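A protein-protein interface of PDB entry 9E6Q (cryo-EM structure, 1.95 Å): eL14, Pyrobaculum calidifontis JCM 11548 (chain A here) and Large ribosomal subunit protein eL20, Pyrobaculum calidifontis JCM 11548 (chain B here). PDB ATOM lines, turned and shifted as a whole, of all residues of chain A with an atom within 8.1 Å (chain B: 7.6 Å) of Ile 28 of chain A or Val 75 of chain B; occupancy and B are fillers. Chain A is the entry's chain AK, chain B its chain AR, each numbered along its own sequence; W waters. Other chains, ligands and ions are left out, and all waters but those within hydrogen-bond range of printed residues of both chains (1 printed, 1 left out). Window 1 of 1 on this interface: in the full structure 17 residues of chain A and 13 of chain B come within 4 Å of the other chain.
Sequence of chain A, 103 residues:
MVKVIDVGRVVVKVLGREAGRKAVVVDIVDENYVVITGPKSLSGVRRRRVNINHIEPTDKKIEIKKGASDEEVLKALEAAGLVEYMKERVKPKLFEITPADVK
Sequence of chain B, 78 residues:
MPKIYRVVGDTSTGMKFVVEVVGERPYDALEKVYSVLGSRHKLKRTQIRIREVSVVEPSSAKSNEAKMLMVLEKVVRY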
ATOM      1  N   VAL A   2      21.934   4.033 -15.300  1.00  0.00           N
ATOM      2  CA  VAL A   2      20.623   4.647 -15.436  1.00  0.00           C
ATOM      3  C   VAL A   2      20.782   6.002 -16.123  1.00  0.00           C
ATOM      4  O   VAL A   2      21.850   6.608 -16.063  1.00  0.00           O
ATOM      5  CB  VAL A   2      19.933   4.773 -14.067  1.00  0.00           C
ATOM      6  CG1 VAL A   2      20.441   5.992 -13.307  1.00  0.00           C
ATOM      7  CG2 VAL A   2      18.422   4.792 -14.224  1.00  0.00           C
ATOM      8  N   LYS A   3      19.730   6.472 -16.789  1.00  0.00           N
ATOM      9  CA  LYS A   3      19.773   7.730 -17.526  1.00  0.00           C
ATOM     10  C   LYS A   3      19.193   8.848 -16.673  1.00  0.00           C
ATOM     11  O   LYS A   3      18.093   8.713 -16.130  1.00  0.00           O
ATOM     12  CB  LYS A   3      19.003   7.622 -18.841  1.00  0.00           C
ATOM     13  CG  LYS A   3      18.401   8.936 -19.295  1.00  0.00           C
ATOM     14  CD  LYS A   3      17.610   8.802 -20.584  1.00  0.00           C
ATOM     15  CE  LYS A   3      18.423   8.199 -21.698  1.00  0.00           C
ATOM     16  NZ  LYS A   3      17.542   7.570 -22.714  1.00  0.00           N
ATOM     17  N   VAL A   4      19.927   9.951 -16.568  1.00  0.00           N
ATOM     18  CA  VAL A   4      19.524  11.100 -15.767  1.00  0.00           C
ATOM     19  C   VAL A   4      19.422  12.308 -16.685  1.00  0.00           C
ATOM     20  O   VAL A   4      20.392  12.661 -17.365  1.00  0.00           O
ATOM     21  CB  VAL A   4      20.511  11.372 -14.623  1.00  0.00           C
ATOM     22  CG1 VAL A   4      20.348  12.787 -14.111  1.00  0.00           C
ATOM     23  CG2 VAL A   4      20.318  10.368 -13.503  1.00  0.00           C
ATOM     24  N   ILE A   5      18.252  12.938 -16.700  1.00  0.00           N
ATOM     25  CA  ILE A   5      18.001  14.152 -17.466  1.00  0.00           C
ATOM     26  C   ILE A   5      17.640  15.243 -16.473  1.00  0.00           C
ATOM     27  O   ILE A   5      16.698  15.085 -15.691  1.00  0.00           O
ATOM     28  CB  ILE A   5      16.873  13.962 -18.492  1.00  0.00           C
ATOM     29  CG1 ILE A   5      17.186  12.808 -19.441  1.00  0.00           C
ATOM     30  CG2 ILE A   5      16.642  15.243 -19.258  1.00  0.00           C
ATOM     31  CD1 ILE A   5      18.470  12.958 -20.180  1.00  0.00           C
ATOM     32  N   ASP A   6      18.376  16.347 -16.507  1.00  0.00           N
ATOM     33  CA  ASP A   6      18.190  17.422 -15.549  1.00  0.00           C
ATOM     34  C   ASP A   6      18.279  18.767 -16.245  1.00  0.00           C
ATOM     35  O   ASP A   6      18.963  18.905 -17.260  1.00  0.00           O
ATOM     36  CB  ASP A   6      19.229  17.331 -14.432  1.00  0.00           C
ATOM     37  CG  ASP A   6      20.590  16.938 -14.949  1.00  0.00           C
ATOM     38  OD1 ASP A   6      20.698  15.850 -15.549  1.00  0.00           O
ATOM     39  OD2 ASP A   6      21.550  17.708 -14.758  1.00  0.00           O
ATOM     40  N   VAL A   7      17.593  19.759 -15.685  1.00  0.00           N
ATOM     41  CA  VAL A   7      17.504  21.085 -16.285  1.00  0.00           C
ATOM     42  C   VAL A   7      18.893  21.695 -16.391  1.00  0.00           C
ATOM     43  O   VAL A   7      19.600  21.842 -15.390  1.00  0.00           O
ATOM     44  CB  VAL A   7      16.557  21.991 -15.481  1.00  0.00           C
ATOM     45  CG1 VAL A   7      16.803  23.446 -15.815  1.00  0.00           C
ATOM     46  CG2 VAL A   7      15.122  21.621 -15.767  1.00  0.00           C
ATOM     47  N   GLY A   8      19.287  22.059 -17.608  1.00  0.00           N
ATOM     48  CA  GLY A   8      20.604  22.573 -17.899  1.00  0.00           C
ATOM     49  C   GLY A   8      21.502  21.597 -18.622  1.00  0.00           C
ATOM     50  O   GLY A   8      22.502  22.017 -19.213  1.00  0.00           O
ATOM     51  N   VAL A  25      18.340  21.017 -22.162  1.00  0.00           N
ATOM     52  CA  VAL A  25      17.094  20.824 -21.431  1.00  0.00           C
ATOM     53  C   VAL A  25      16.800  22.091 -20.644  1.00  0.00           C
ATOM     54  O   VAL A  25      17.639  22.559 -19.870  1.00  0.00           O
ATOM     55  CB  VAL A  25      17.179  19.610 -20.497  1.00  0.00           C
ATOM     56  CG1 VAL A  25      15.893  19.459 -19.716  1.00  0.00           C
ATOM     57  CG2 VAL A  25      17.485  18.359 -21.278  1.00  0.00           C
ATOM     58  N   VAL A  26      15.605  22.645 -20.830  1.00  0.00           N
ATOM     59  CA  VAL A  26      15.227  23.890 -20.172  1.00  0.00           C
ATOM     60  C   VAL A  26      14.029  23.745 -19.258  1.00  0.00           C
ATOM     61  O   VAL A  26      13.725  24.693 -18.519  1.00  0.00           O
ATOM     62  CB  VAL A  26      14.966  25.013 -21.194  1.00  0.00           C
ATOM     63  CG1 VAL A  26      16.264  25.440 -21.807  1.00  0.00           C
ATOM     64  CG2 VAL A  26      13.982  24.557 -22.252  1.00  0.00           C
ATOM     65  N   ASP A  27      13.335  22.615 -19.281  1.00  0.00           N
ATOM     66  CA  ASP A  27      12.215  22.417 -18.376  1.00  0.00           C
ATOM     67  C   ASP A  27      11.868  20.940 -18.330  1.00  0.00           C
ATOM     68  O   ASP A  27      12.284  20.159 -19.188  1.00  0.00           O
ATOM     69  CB  ASP A  27      10.998  23.239 -18.797  1.00  0.00           C
ATOM     70  CG  ASP A  27      10.069  23.519 -17.647  1.00  0.00           C
ATOM     71  OD1 ASP A  27       9.993  22.677 -16.733  1.00  0.00           O
ATOM     72  OD2 ASP A  27       9.421  24.582 -17.649  1.00  0.00           O
ATOM     73  N   ILE A  28      11.097  20.572 -17.314  1.00  0.00           N
ATOM     74  CA  ILE A  28      10.577  19.223 -17.147  1.00  0.00           C
ATOM     75  C   ILE A  28       9.063  19.285 -17.262  1.00  0.00           C
ATOM     76  O   ILE A  28       8.416  20.062 -16.553  1.00  0.00           O
ATOM     77  CB  ILE A  28      10.997  18.623 -15.795  1.00  0.00           C
ATOM     78  CG1 ILE A  28      12.502  18.774 -15.589  1.00  0.00           C
ATOM     79  CG2 ILE A  28      10.569  17.173 -15.701  1.00  0.00           C
ATOM     80  CD1 ILE A  28      13.311  17.645 -16.147  1.00  0.00           C
ATOM     81  N   VAL A  29       8.497  18.478 -18.156  1.00  0.00           N
ATOM     82  CA  VAL A  29       7.043  18.393 -18.266  1.00  0.00           C
ATOM     83  C   VAL A  29       6.489  17.400 -17.254  1.00  0.00           C
ATOM     84  O   VAL A  29       5.721  17.760 -16.357  1.00  0.00           O
ATOM     85  CB  VAL A  29       6.632  18.018 -19.698  1.00  0.00           C
ATOM     86  CG1 VAL A  29       5.126  18.082 -19.846  1.00  0.00           C
ATOM     87  CG2 VAL A  29       7.308  18.927 -20.690  1.00  0.00           C
ATOM     88  N   ASP A  30       6.877  16.139 -17.380  1.00  0.00           N
ATOM     89  CA  ASP A  30       6.513  15.110 -16.417  1.00  0.00           C
ATOM     90  C   ASP A  30       7.673  14.127 -16.347  1.00  0.00           C
ATOM     91  O   ASP A  30       8.800  14.454 -16.729  1.00  0.00           O
ATOM     92  CB  ASP A  30       5.177  14.442 -16.787  1.00  0.00           C
ATOM     93  CG  ASP A  30       5.127  13.967 -18.225  1.00  0.00           C
ATOM     94  OD1 ASP A  30       6.123  13.405 -18.720  1.00  0.00           O
ATOM     95  OD2 ASP A  30       4.067  14.138 -18.859  1.00  0.00           O
ATOM     96  N   GLU A  31       7.408  12.928 -15.841  1.00  0.00           N
ATOM     97  CA  GLU A  31       8.451  11.918 -15.763  1.00  0.00           C
ATOM     98  C   GLU A  31       8.868  11.389 -17.129  1.00  0.00           C
ATOM     99  O   GLU A  31       9.867  10.670 -17.212  1.00  0.00           O
ATOM    100  CB  GLU A  31       7.984  10.762 -14.887  1.00  0.00           C
ATOM    101  CG  GLU A  31       7.225  11.206 -13.656  1.00  0.00           C
ATOM    102  CD  GLU A  31       8.003  10.995 -12.379  1.00  0.00           C
ATOM    103  OE1 GLU A  31       7.374  10.681 -11.348  1.00  0.00           O
ATOM    104  OE2 GLU A  31       9.241  11.150 -12.400  1.00  0.00           O
ATOM    105  N   ASN A  32       8.140  11.712 -18.193  1.00  0.00           N
ATOM    106  CA  ASN A  32       8.427  11.151 -19.505  1.00  0.00           C
ATOM    107  C   ASN A  32       8.869  12.169 -20.541  1.00  0.00           C
ATOM    108  O   ASN A  32       9.569  11.797 -21.479  1.00  0.00           O
ATOM    109  CB  ASN A  32       7.197  10.410 -20.039  1.00  0.00           C
ATOM    110  CG  ASN A  32       6.828   9.217 -19.193  1.00  0.00           C
ATOM    111  OD1 ASN A  32       7.669   8.381 -18.885  1.00  0.00           O
ATOM    112  ND2 ASN A  32       5.565   9.127 -18.818  1.00  0.00           N
ATOM    113  N   TYR A  33       8.481  13.432 -20.408  1.00  0.00           N
ATOM    114  CA  TYR A  33       8.782  14.451 -21.400  1.00  0.00           C
ATOM    115  C   TYR A  33       9.503  15.625 -20.755  1.00  0.00           C
ATOM    116  O   TYR A  33       9.211  15.999 -19.619  1.00  0.00           O
ATOM    117  CB  TYR A  33       7.507  14.964 -22.076  1.00  0.00           C
ATOM    118  CG  TYR A  33       6.906  14.051 -23.115  1.00  0.00           C
ATOM    119  CD1 TYR A  33       6.068  13.008 -22.757  1.00  0.00           C
ATOM    120  CD2 TYR A  33       7.157  14.251 -24.461  1.00  0.00           C
ATOM    121  CE1 TYR A  33       5.513  12.185 -23.706  1.00  0.00           C
ATOM    122  CE2 TYR A  33       6.602  13.438 -25.414  1.00  0.00           C
ATOM    123  CZ  TYR A  33       5.783  12.408 -25.033  1.00  0.00           C
ATOM    124  OH  TYR A  33       5.235  11.597 -25.988  1.00  0.00           O
ATOM    125  N   VAL A  34      10.437  16.215 -21.501  1.00  0.00           N
ATOM    126  CA  VAL A  34      11.104  17.452 -21.116  1.00  0.00           C
ATOM    127  C   VAL A  34      11.043  18.416 -22.290  1.00  0.00           C
ATOM    128  O   VAL A  34      10.679  18.048 -23.404  1.00  0.00           O
ATOM    129  CB  VAL A  34      12.568  17.237 -20.688  1.00  0.00           C
ATOM    130  CG1 VAL A  34      12.649  16.264 -19.552  1.00  0.00           C
ATOM    131  CG2 VAL A  34      13.405  16.782 -21.863  1.00  0.00           C
ATOM    132  N   VAL A  35      11.414  19.665 -22.027  1.00  0.00           N
ATOM    133  CA  VAL A  35      11.491  20.707 -23.043  1.00  0.00           C
ATOM    134  C   VAL A  35      12.956  20.960 -23.351  1.00  0.00           C
ATOM    135  O   VAL A  35      13.755  21.195 -22.441  1.00  0.00           O
ATOM    136  CB  VAL A  35      10.808  22.002 -22.590  1.00  0.00           C
ATOM    137  CG1 VAL A  35      10.828  23.015 -23.709  1.00  0.00           C
ATOM    138  CG2 VAL A  35       9.397  21.728 -22.144  1.00  0.00           C
ATOM    139  N   ILE A  36      13.312  20.916 -24.628  1.00  0.00           N
ATOM    140  CA  ILE A  36      14.664  21.206 -25.078  1.00  0.00           C
ATOM    141  C   ILE A  36      14.614  22.350 -26.077  1.00  0.00           C
ATOM    142  O   ILE A  36      13.714  22.416 -26.918  1.00  0.00           O
ATOM    143  CB  ILE A  36      15.347  19.975 -25.707  1.00  0.00           C
ATOM    144  CG1 ILE A  36      14.552  19.473 -26.910  1.00  0.00           C
ATOM    145  CG2 ILE A  36      15.528  18.887 -24.678  1.00  0.00           C
ATOM    146  CD1 ILE A  36      15.314  18.532 -27.785  1.00  0.00           C
ATOM    147  N   ILE A  52      11.928  11.449 -23.226  1.00  0.00           N
ATOM    148  CA  ILE A  52      13.227  11.102 -22.659  1.00  0.00           C
ATOM    149  C   ILE A  52      13.902   9.999 -23.459  1.00  0.00           C
ATOM    150  O   ILE A  52      15.129   9.978 -23.585  1.00  0.00           O
ATOM    151  CB  ILE A  52      13.057  10.710 -21.181  1.00  0.00           C
ATOM    152  CG1 ILE A  52      12.560  11.907 -20.392  1.00  0.00           C
ATOM    153  CG2 ILE A  52      14.360  10.256 -20.598  1.00  0.00           C
ATOM    154  CD1 ILE A  52      13.554  13.009 -20.376  1.00  0.00           C
ATOM    155  N   ILE A  55      16.443  11.242 -26.338  1.00  0.00           N
ATOM    156  CA  ILE A  55      17.621  12.058 -26.084  1.00  0.00           C
ATOM    157  C   ILE A  55      18.595  11.261 -25.234  1.00  0.00           C
ATOM    158  O   ILE A  55      18.203  10.365 -24.481  1.00  0.00           O
ATOM    159  CB  ILE A  55      17.269  13.393 -25.395  1.00  0.00           C
ATOM    160  CG1 ILE A  55      16.353  13.154 -24.200  1.00  0.00           C
ATOM    161  CG2 ILE A  55      16.630  14.351 -26.374  1.00  0.00           C
ATOM    162  CD1 ILE A  55      16.001  14.403 -23.453  1.00  0.00           C
ATOM    163  N   PRO A  57      21.956  12.069 -22.588  1.00  0.00           N
ATOM    164  CA  PRO A  57      22.725  13.131 -21.941  1.00  0.00           C
ATOM    165  C   PRO A  57      24.190  13.076 -22.332  1.00  0.00           C
ATOM    166  O   PRO A  57      24.759  12.009 -22.569  1.00  0.00           O
ATOM    167  CB  PRO A  57      22.545  12.850 -20.444  1.00  0.00           C
ATOM    168  CG  PRO A  57      21.735  11.607 -20.338  1.00  0.00           C
ATOM    169  CD  PRO A  57      21.650  10.964 -21.674  1.00  0.00           C
ATOM    170  N   LYS A  66      14.347  27.139 -14.577  1.00  0.00           N
ATOM    171  CA  LYS A  66      13.308  26.369 -15.245  1.00  0.00           C
ATOM    172  C   LYS A  66      12.575  27.241 -16.253  1.00  0.00           C
ATOM    173  O   LYS A  66      12.210  28.381 -15.956  1.00  0.00           O
ATOM    174  CB  LYS A  66      12.324  25.805 -14.226  1.00  0.00           C
ATOM    175  CG  LYS A  66      12.554  24.351 -13.893  1.00  0.00           C
ATOM    176  CD  LYS A  66      12.112  24.054 -12.478  1.00  0.00           C
ATOM    177  CE  LYS A  66      10.684  23.563 -12.422  1.00  0.00           C
ATOM    178  NZ  LYS A  66      10.464  22.381 -13.288  1.00  0.00           N
ATOM    179  N   GLY A  67      12.353  26.696 -17.444  1.00  0.00           N
ATOM    180  CA  GLY A  67      11.726  27.459 -18.504  1.00  0.00           C
ATOM    181  C   GLY A  67      12.553  28.621 -18.993  1.00  0.00           C
ATOM    182  O   GLY A  67      11.995  29.656 -19.364  1.00  0.00           O
ATOM    183  N   PRO B   2       4.903  24.116 -18.630  1.00  0.00           N
ATOM    184  CA  PRO B   2       4.137  23.100 -17.909  1.00  0.00           C
ATOM    185  C   PRO B   2       3.062  23.724 -17.041  1.00  0.00           C
ATOM    186  O   PRO B   2       3.314  24.703 -16.352  1.00  0.00           O
ATOM    187  CB  PRO B   2       5.184  22.390 -17.049  1.00  0.00           C
ATOM    188  CG  PRO B   2       6.495  23.018 -17.361  1.00  0.00           C
ATOM    189  CD  PRO B   2       6.353  23.891 -18.550  1.00  0.00           C
ATOM    190  N   LYS B   3       1.861  23.163 -17.100  1.00  0.00           N
ATOM    191  CA  LYS B   3       0.740  23.642 -16.313  1.00  0.00           C
ATOM    192  C   LYS B   3      -0.071  22.448 -15.848  1.00  0.00           C
ATOM    193  O   LYS B   3      -0.009  21.366 -16.434  1.00  0.00           O
ATOM    194  CB  LYS B   3      -0.152  24.602 -17.105  1.00  0.00           C
ATOM    195  CG  LYS B   3       0.552  25.832 -17.620  1.00  0.00           C
ATOM    196  CD  LYS B   3      -0.357  26.642 -18.513  1.00  0.00           C
ATOM    197  CE  LYS B   3       0.406  27.745 -19.213  1.00  0.00           C
ATOM    198  NZ  LYS B   3       1.865  27.679 -18.936  1.00  0.00           N
ATOM    199  N   VAL B  22      -0.761  17.197 -15.767  1.00  0.00           N
ATOM    200  CA  VAL B  22       0.296  18.153 -16.057  1.00  0.00           C
ATOM    201  C   VAL B  22       0.726  17.980 -17.505  1.00  0.00           C
ATOM    202  O   VAL B  22       1.023  16.866 -17.947  1.00  0.00           O
ATOM    203  CB  VAL B  22       1.484  17.967 -15.102  1.00  0.00           C
ATOM    204  CG1 VAL B  22       2.576  18.950 -15.431  1.00  0.00           C
ATOM    205  CG2 VAL B  22       1.028  18.144 -13.676  1.00  0.00           C
ATOM    206  N   GLU B  24       2.266  20.345 -21.294  1.00  0.00           N
ATOM    207  CA  GLU B  24       2.711  21.577 -21.928  1.00  0.00           C
ATOM    208  C   GLU B  24       1.542  22.383 -22.476  1.00  0.00           C
ATOM    209  O   GLU B  24       1.475  23.599 -22.278  1.00  0.00           O
ATOM    210  CB  GLU B  24       3.701  21.248 -23.042  1.00  0.00           C
ATOM    211  CG  GLU B  24       4.522  22.420 -23.492  1.00  0.00           C
ATOM    212  CD  GLU B  24       5.828  22.505 -22.756  1.00  0.00           C
ATOM    213  OE1 GLU B  24       6.254  21.467 -22.221  1.00  0.00           O
ATOM    214  OE2 GLU B  24       6.424  23.603 -22.701  1.00  0.00           O
ATOM    215  N   LEU B  69       5.223  17.254  -9.743  1.00  0.00           N
ATOM    216  CA  LEU B  69       5.758  17.328 -11.100  1.00  0.00           C
ATOM    217  C   LEU B  69       6.133  18.755 -11.470  1.00  0.00           C
ATOM    218  O   LEU B  69       7.115  18.979 -12.182  1.00  0.00           O
ATOM    219  CB  LEU B  69       4.753  16.768 -12.105  1.00  0.00           C
ATOM    220  CG  LEU B  69       4.341  15.311 -11.942  1.00  0.00           C
ATOM    221  CD1 LEU B  69       3.222  14.974 -12.905  1.00  0.00           C
ATOM    222  CD2 LEU B  69       5.525  14.400 -12.158  1.00  0.00           C
ATOM    223  N   MET B  70       5.373  19.734 -10.980  1.00  0.00           N
ATOM    224  CA  MET B  70       5.611  21.124 -11.348  1.00  0.00           C
ATOM    225  C   MET B  70       6.990  21.613 -10.940  1.00  0.00           C
ATOM    226  O   MET B  70       7.567  22.467 -11.618  1.00  0.00           O
ATOM    227  CB  MET B  70       4.548  22.015 -10.721  1.00  0.00           C
ATOM    228  CG  MET B  70       3.238  21.961 -11.423  1.00  0.00           C
ATOM    229  SD  MET B  70       3.483  22.082 -13.195  1.00  0.00           S
ATOM    230  CE  MET B  70       2.702  23.655 -13.476  1.00  0.00           C
ATOM    231  N   VAL B  71       7.532  21.102  -9.838  1.00  0.00           N
ATOM    232  CA  VAL B  71       8.797  21.583  -9.303  1.00  0.00           C
ATOM    233  C   VAL B  71       9.943  20.632  -9.615  1.00  0.00           C
ATOM    234  O   VAL B  71      11.037  20.788  -9.067  1.00  0.00           O
ATOM    235  CB  VAL B  71       8.699  21.843  -7.795  1.00  0.00           C
ATOM    236  CG1 VAL B  71       7.543  22.771  -7.503  1.00  0.00           C
ATOM    237  CG2 VAL B  71       8.522  20.540  -7.051  1.00  0.00           C
ATOM    238  N   LEU B  72       9.721  19.651 -10.485  1.00  0.00           N
ATOM    239  CA  LEU B  72      10.762  18.690 -10.814  1.00  0.00           C
ATOM    240  C   LEU B  72      11.943  19.386 -11.474  1.00  0.00           C
ATOM    241  O   LEU B  72      11.770  20.220 -12.365  1.00  0.00           O
ATOM    242  CB  LEU B  72      10.200  17.612 -11.740  1.00  0.00           C
ATOM    243  CG  LEU B  72      10.386  16.160 -11.310  1.00  0.00           C
ATOM    244  CD1 LEU B  72      10.222  16.039  -9.809  1.00  0.00           C
ATOM    245  CD2 LEU B  72       9.395  15.278 -12.028  1.00  0.00           C
ATOM    246  N   GLU B  73      13.148  19.043 -11.030  1.00  0.00           N
ATOM    247  CA  GLU B  73      14.366  19.544 -11.645  1.00  0.00           C
ATOM    248  C   GLU B  73      15.104  18.484 -12.446  1.00  0.00           C
ATOM    249  O   GLU B  73      15.995  18.829 -13.226  1.00  0.00           O
ATOM    250  CB  GLU B  73      15.307  20.112 -10.577  1.00  0.00           C
ATOM    251  CG  GLU B  73      14.793  21.355  -9.873  1.00  0.00           C
ATOM    252  CD  GLU B  73      15.342  22.637 -10.467  1.00  0.00           C
ATOM    253  OE1 GLU B  73      16.546  22.679 -10.793  1.00  0.00           O
ATOM    254  OE2 GLU B  73      14.574  23.612 -10.589  1.00  0.00           O
ATOM    255  N   LYS B  74      14.760  17.210 -12.275  1.00  0.00           N
ATOM    256  CA  LYS B  74      15.435  16.142 -12.992  1.00  0.00           C
ATOM    257  C   LYS B  74      14.535  14.919 -13.042  1.00  0.00           C
ATOM    258  O   LYS B  74      13.627  14.758 -12.226  1.00  0.00           O
ATOM    259  CB  LYS B  74      16.771  15.788 -12.341  1.00  0.00           C
ATOM    260  CG  LYS B  74      16.667  15.471 -10.866  1.00  0.00           C
ATOM    261  CD  LYS B  74      18.038  15.207 -10.281  1.00  0.00           C
ATOM    262  CE  LYS B  74      18.403  13.742 -10.382  1.00  0.00           C
ATOM    263  NZ  LYS B  74      17.283  12.887  -9.920  1.00  0.00           N
ATOM    264  N   VAL B  75      14.812  14.055 -14.012  1.00  0.00           N
ATOM    265  CA  VAL B  75      14.093  12.801 -14.182  1.00  0.00           C
ATOM    266  C   VAL B  75      15.112  11.694 -14.394  1.00  0.00           C
ATOM    267  O   VAL B  75      16.241  11.936 -14.828  1.00  0.00           O
ATOM    268  CB  VAL B  75      13.096  12.852 -15.360  1.00  0.00           C
ATOM    269  CG1 VAL B  75      11.910  13.722 -15.012  1.00  0.00           C
ATOM    270  CG2 VAL B  75      13.778  13.369 -16.595  1.00  0.00           C
ATOM    271  N   VAL B  76      14.706  10.469 -14.080  1.00  0.00           N
ATOM    272  CA  VAL B  76      15.561   9.295 -14.182  1.00  0.00           C
ATOM    273  C   VAL B  76      14.822   8.231 -14.980  1.00  0.00           C
ATOM    274  O   VAL B  76      13.627   8.006 -14.762  1.00  0.00           O
ATOM    275  CB  VAL B  76      15.950   8.752 -12.798  1.00  0.00           C
ATOM    276  CG1 VAL B  76      16.990   7.680 -12.937  1.00  0.00           C
ATOM    277  CG2 VAL B  76      16.456   9.874 -11.905  1.00  0.00           C
ATOM    278  N   ARG B  77      15.521   7.586 -15.907  1.00  0.00           N
ATOM    279  CA  ARG B  77      14.918   6.504 -16.671  1.00  0.00           C
ATOM    280  C   ARG B  77      15.749   5.230 -16.574  1.00  0.00           C
ATOM    281  O   ARG B  77      16.865   5.161 -17.088  1.00  0.00           O
ATOM    282  CB  ARG B  77      14.743   6.912 -18.131  1.00  0.00           C
ATOM    283  CG  ARG B  77      13.624   6.178 -18.841  1.00  0.00           C
ATOM    284  CD  ARG B  77      12.813   7.138 -19.682  1.00  0.00           C
ATOM    285  NE  ARG B  77      11.713   6.486 -20.381  1.00  0.00           N
ATOM    286  CZ  ARG B  77      10.457   6.902 -20.336  1.00  0.00           C
ATOM    287  NH1 ARG B  77      10.101   7.948 -19.611  1.00  0.00           N
ATOM    288  NH2 ARG B  77       9.533   6.249 -21.035  1.00  0.00           N
HETATM  289  O   HOH W   1      11.171   8.410 -16.123  1.00  0.00           O
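Printed residues of chain A that touch a printed residue of chain B: Val 2, Lys 3, Val 4, Ile 5, Asp 6, Val 7, Asp 27, Ile 28, Val 29, Asp 30, Glu 31, Asn 32, Val 35, Ile 52 and Lys 66. Hydrophobic or aromatic side chains of chain A within 4 Å of the printed part of chain B: Val 2, Ile 5, Val 7, Ile 28, Val 29, Val 35 and Ile 52. Along chain A the printed residues that touch a printed residue of chain B span positions 2 to 66. Hydrophobic or aromatic side chains of chain B within 4 Å of the printed part of chain A: Pro 2, Val 22, Leu 69, Val 75 and Val 76. Among the printed residues, no Asp or Glu carboxylate lies within 4 Å of a Lys or Arg side-chain nitrogen of the other chain.
The backbone carbonyl oxygen (O) of Ile 55 of chain A is in hydrogen-bond range of the side-chain amino group (NZ) of Lys 3 of chain A (3.4 Å). O of Asp 27 of chain A is in hydrogen-bond range of N of Val 35 of chain A (3.0 Å). The side-chain carboxylate (OD1) of Asp 27 of chain A lies within salt-bridge range of the side-chain amino group (NZ) of Lys 66 of chain A (3.5 Å). OD1 of Asp 30 of chain A lies within hydrogen-bond range of N of Asn 32 of chain A, at 2.7 Å. OD1 of Asp 30 of chain A sits at hydrogen-bond distance from N of Tyr 33 of chain A (2.9 Å). N of Ile 52 of chain A is in hydrogen-bond range of O of Asn 32 of chain A (3.0 Å).
Ile 28 of chain A touches just these residues of chain B: Pro 2, Leu 72 and Val 75. Val 75 of chain B touches seven residues of chain A. Of the printed residues of chain B, Val 7 of chain A touches Glu 73 (3.1 Å). Of the printed residues of chain B, Val 29 of chain A touches Val 22 and Glu 24. Of the printed residues of chain A, Met 70 of chain B touches Lys 66. The nearest printed residue of chain B that does not touch Ile 28 of chain A is Lys 74 of chain B (4.1 Å).
Water W1 bridges the backbone carbonyl oxygen of Glu 31 of chain A (2.8 Å) and the backbone carbonyl oxygen of Val 76 of chain B (2.8 Å).
N of Arg 77 of chain B lies within hydrogen-bond range of O of Lys 3 of chain A (2.8 Å). O of Ile 5 of chain A lies within hydrogen-bond range of N of Val 75 of chain B. O of Glu 73 of chain B lies within hydrogen-bond range of N of Val 7 of chain A, at 3.1 Å. The side-chain amide oxygen of Asn 32 of chain A is in hydrogen-bond range of the guanidinium group of Arg 77 of chain B (2.6 Å). The side-chain amino group (NZ) of Lys 66 of chain A is in hydrogen-bond range of the backbone carbonyl oxygen (O) of Met 70 of chain B (3.3 Å). The backbone carbonyl oxygen (O) of Leu 72 of chain B lies within hydrogen-bond range of the side-chain amino group (NZ) of Lys 66 of chain A, at 2.7 Å.
Among the printed residues, merely in contact across the chains: Lys 66 of chain A with Glu 73 of chain B (3.1 Å), Val 29 of chain A with Glu 24 of chain B (3.1 Å), Val 35 of chain A with Glu 24 of chain B (3.2 Å), Ile 5 of chain A with Lys 74 of chain B (3.2 Å), Lys 3 of chain A with Val 76 of chain B (3.2 Å), Asp 27 of chain A with Pro 2 of chain B (3.3 Å), Val 2 of chain A with Arg 77 of chain B (3.3 Å), Val 2 of chain A with Val 76 of chain B (3.5 Å), Val 29 of chain A with Val 22 of chain B (3.5 Å), Asp 6 of chain A with Glu 73 of chain B (3.5 Å), Val 4 of chain A with Val 75 of chain B (3.5 Å), Asp 6 of chain A with Lys 74 of chain B (3.6 Å), Ile 52 of chain A with Arg 77 of chain B (3.6 Å), Ile 28 of chain A with Leu 72 of chain B (3.6 Å), Ile 28 of chain A with Pro 2 of chain B (3.6 Å), Asp 30 of chain A with Val 75 of chain B (3.6 Å), Glu 31 of chain A with Arg 77 of chain B (3.6 Å), Ile 28 of chain A with Val 75 of chain B (3.8 Å), Ile 52 of chain A with Val 75 of chain B (3.8 Å), Glu 31 of chain A with Leu 69 of chain B (3.9 Å), Lys 3 of chain A with Val 75 of chain B (3.9 Å) and Glu 31 of chain A with Val 75 of chain B (3.97 Å).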
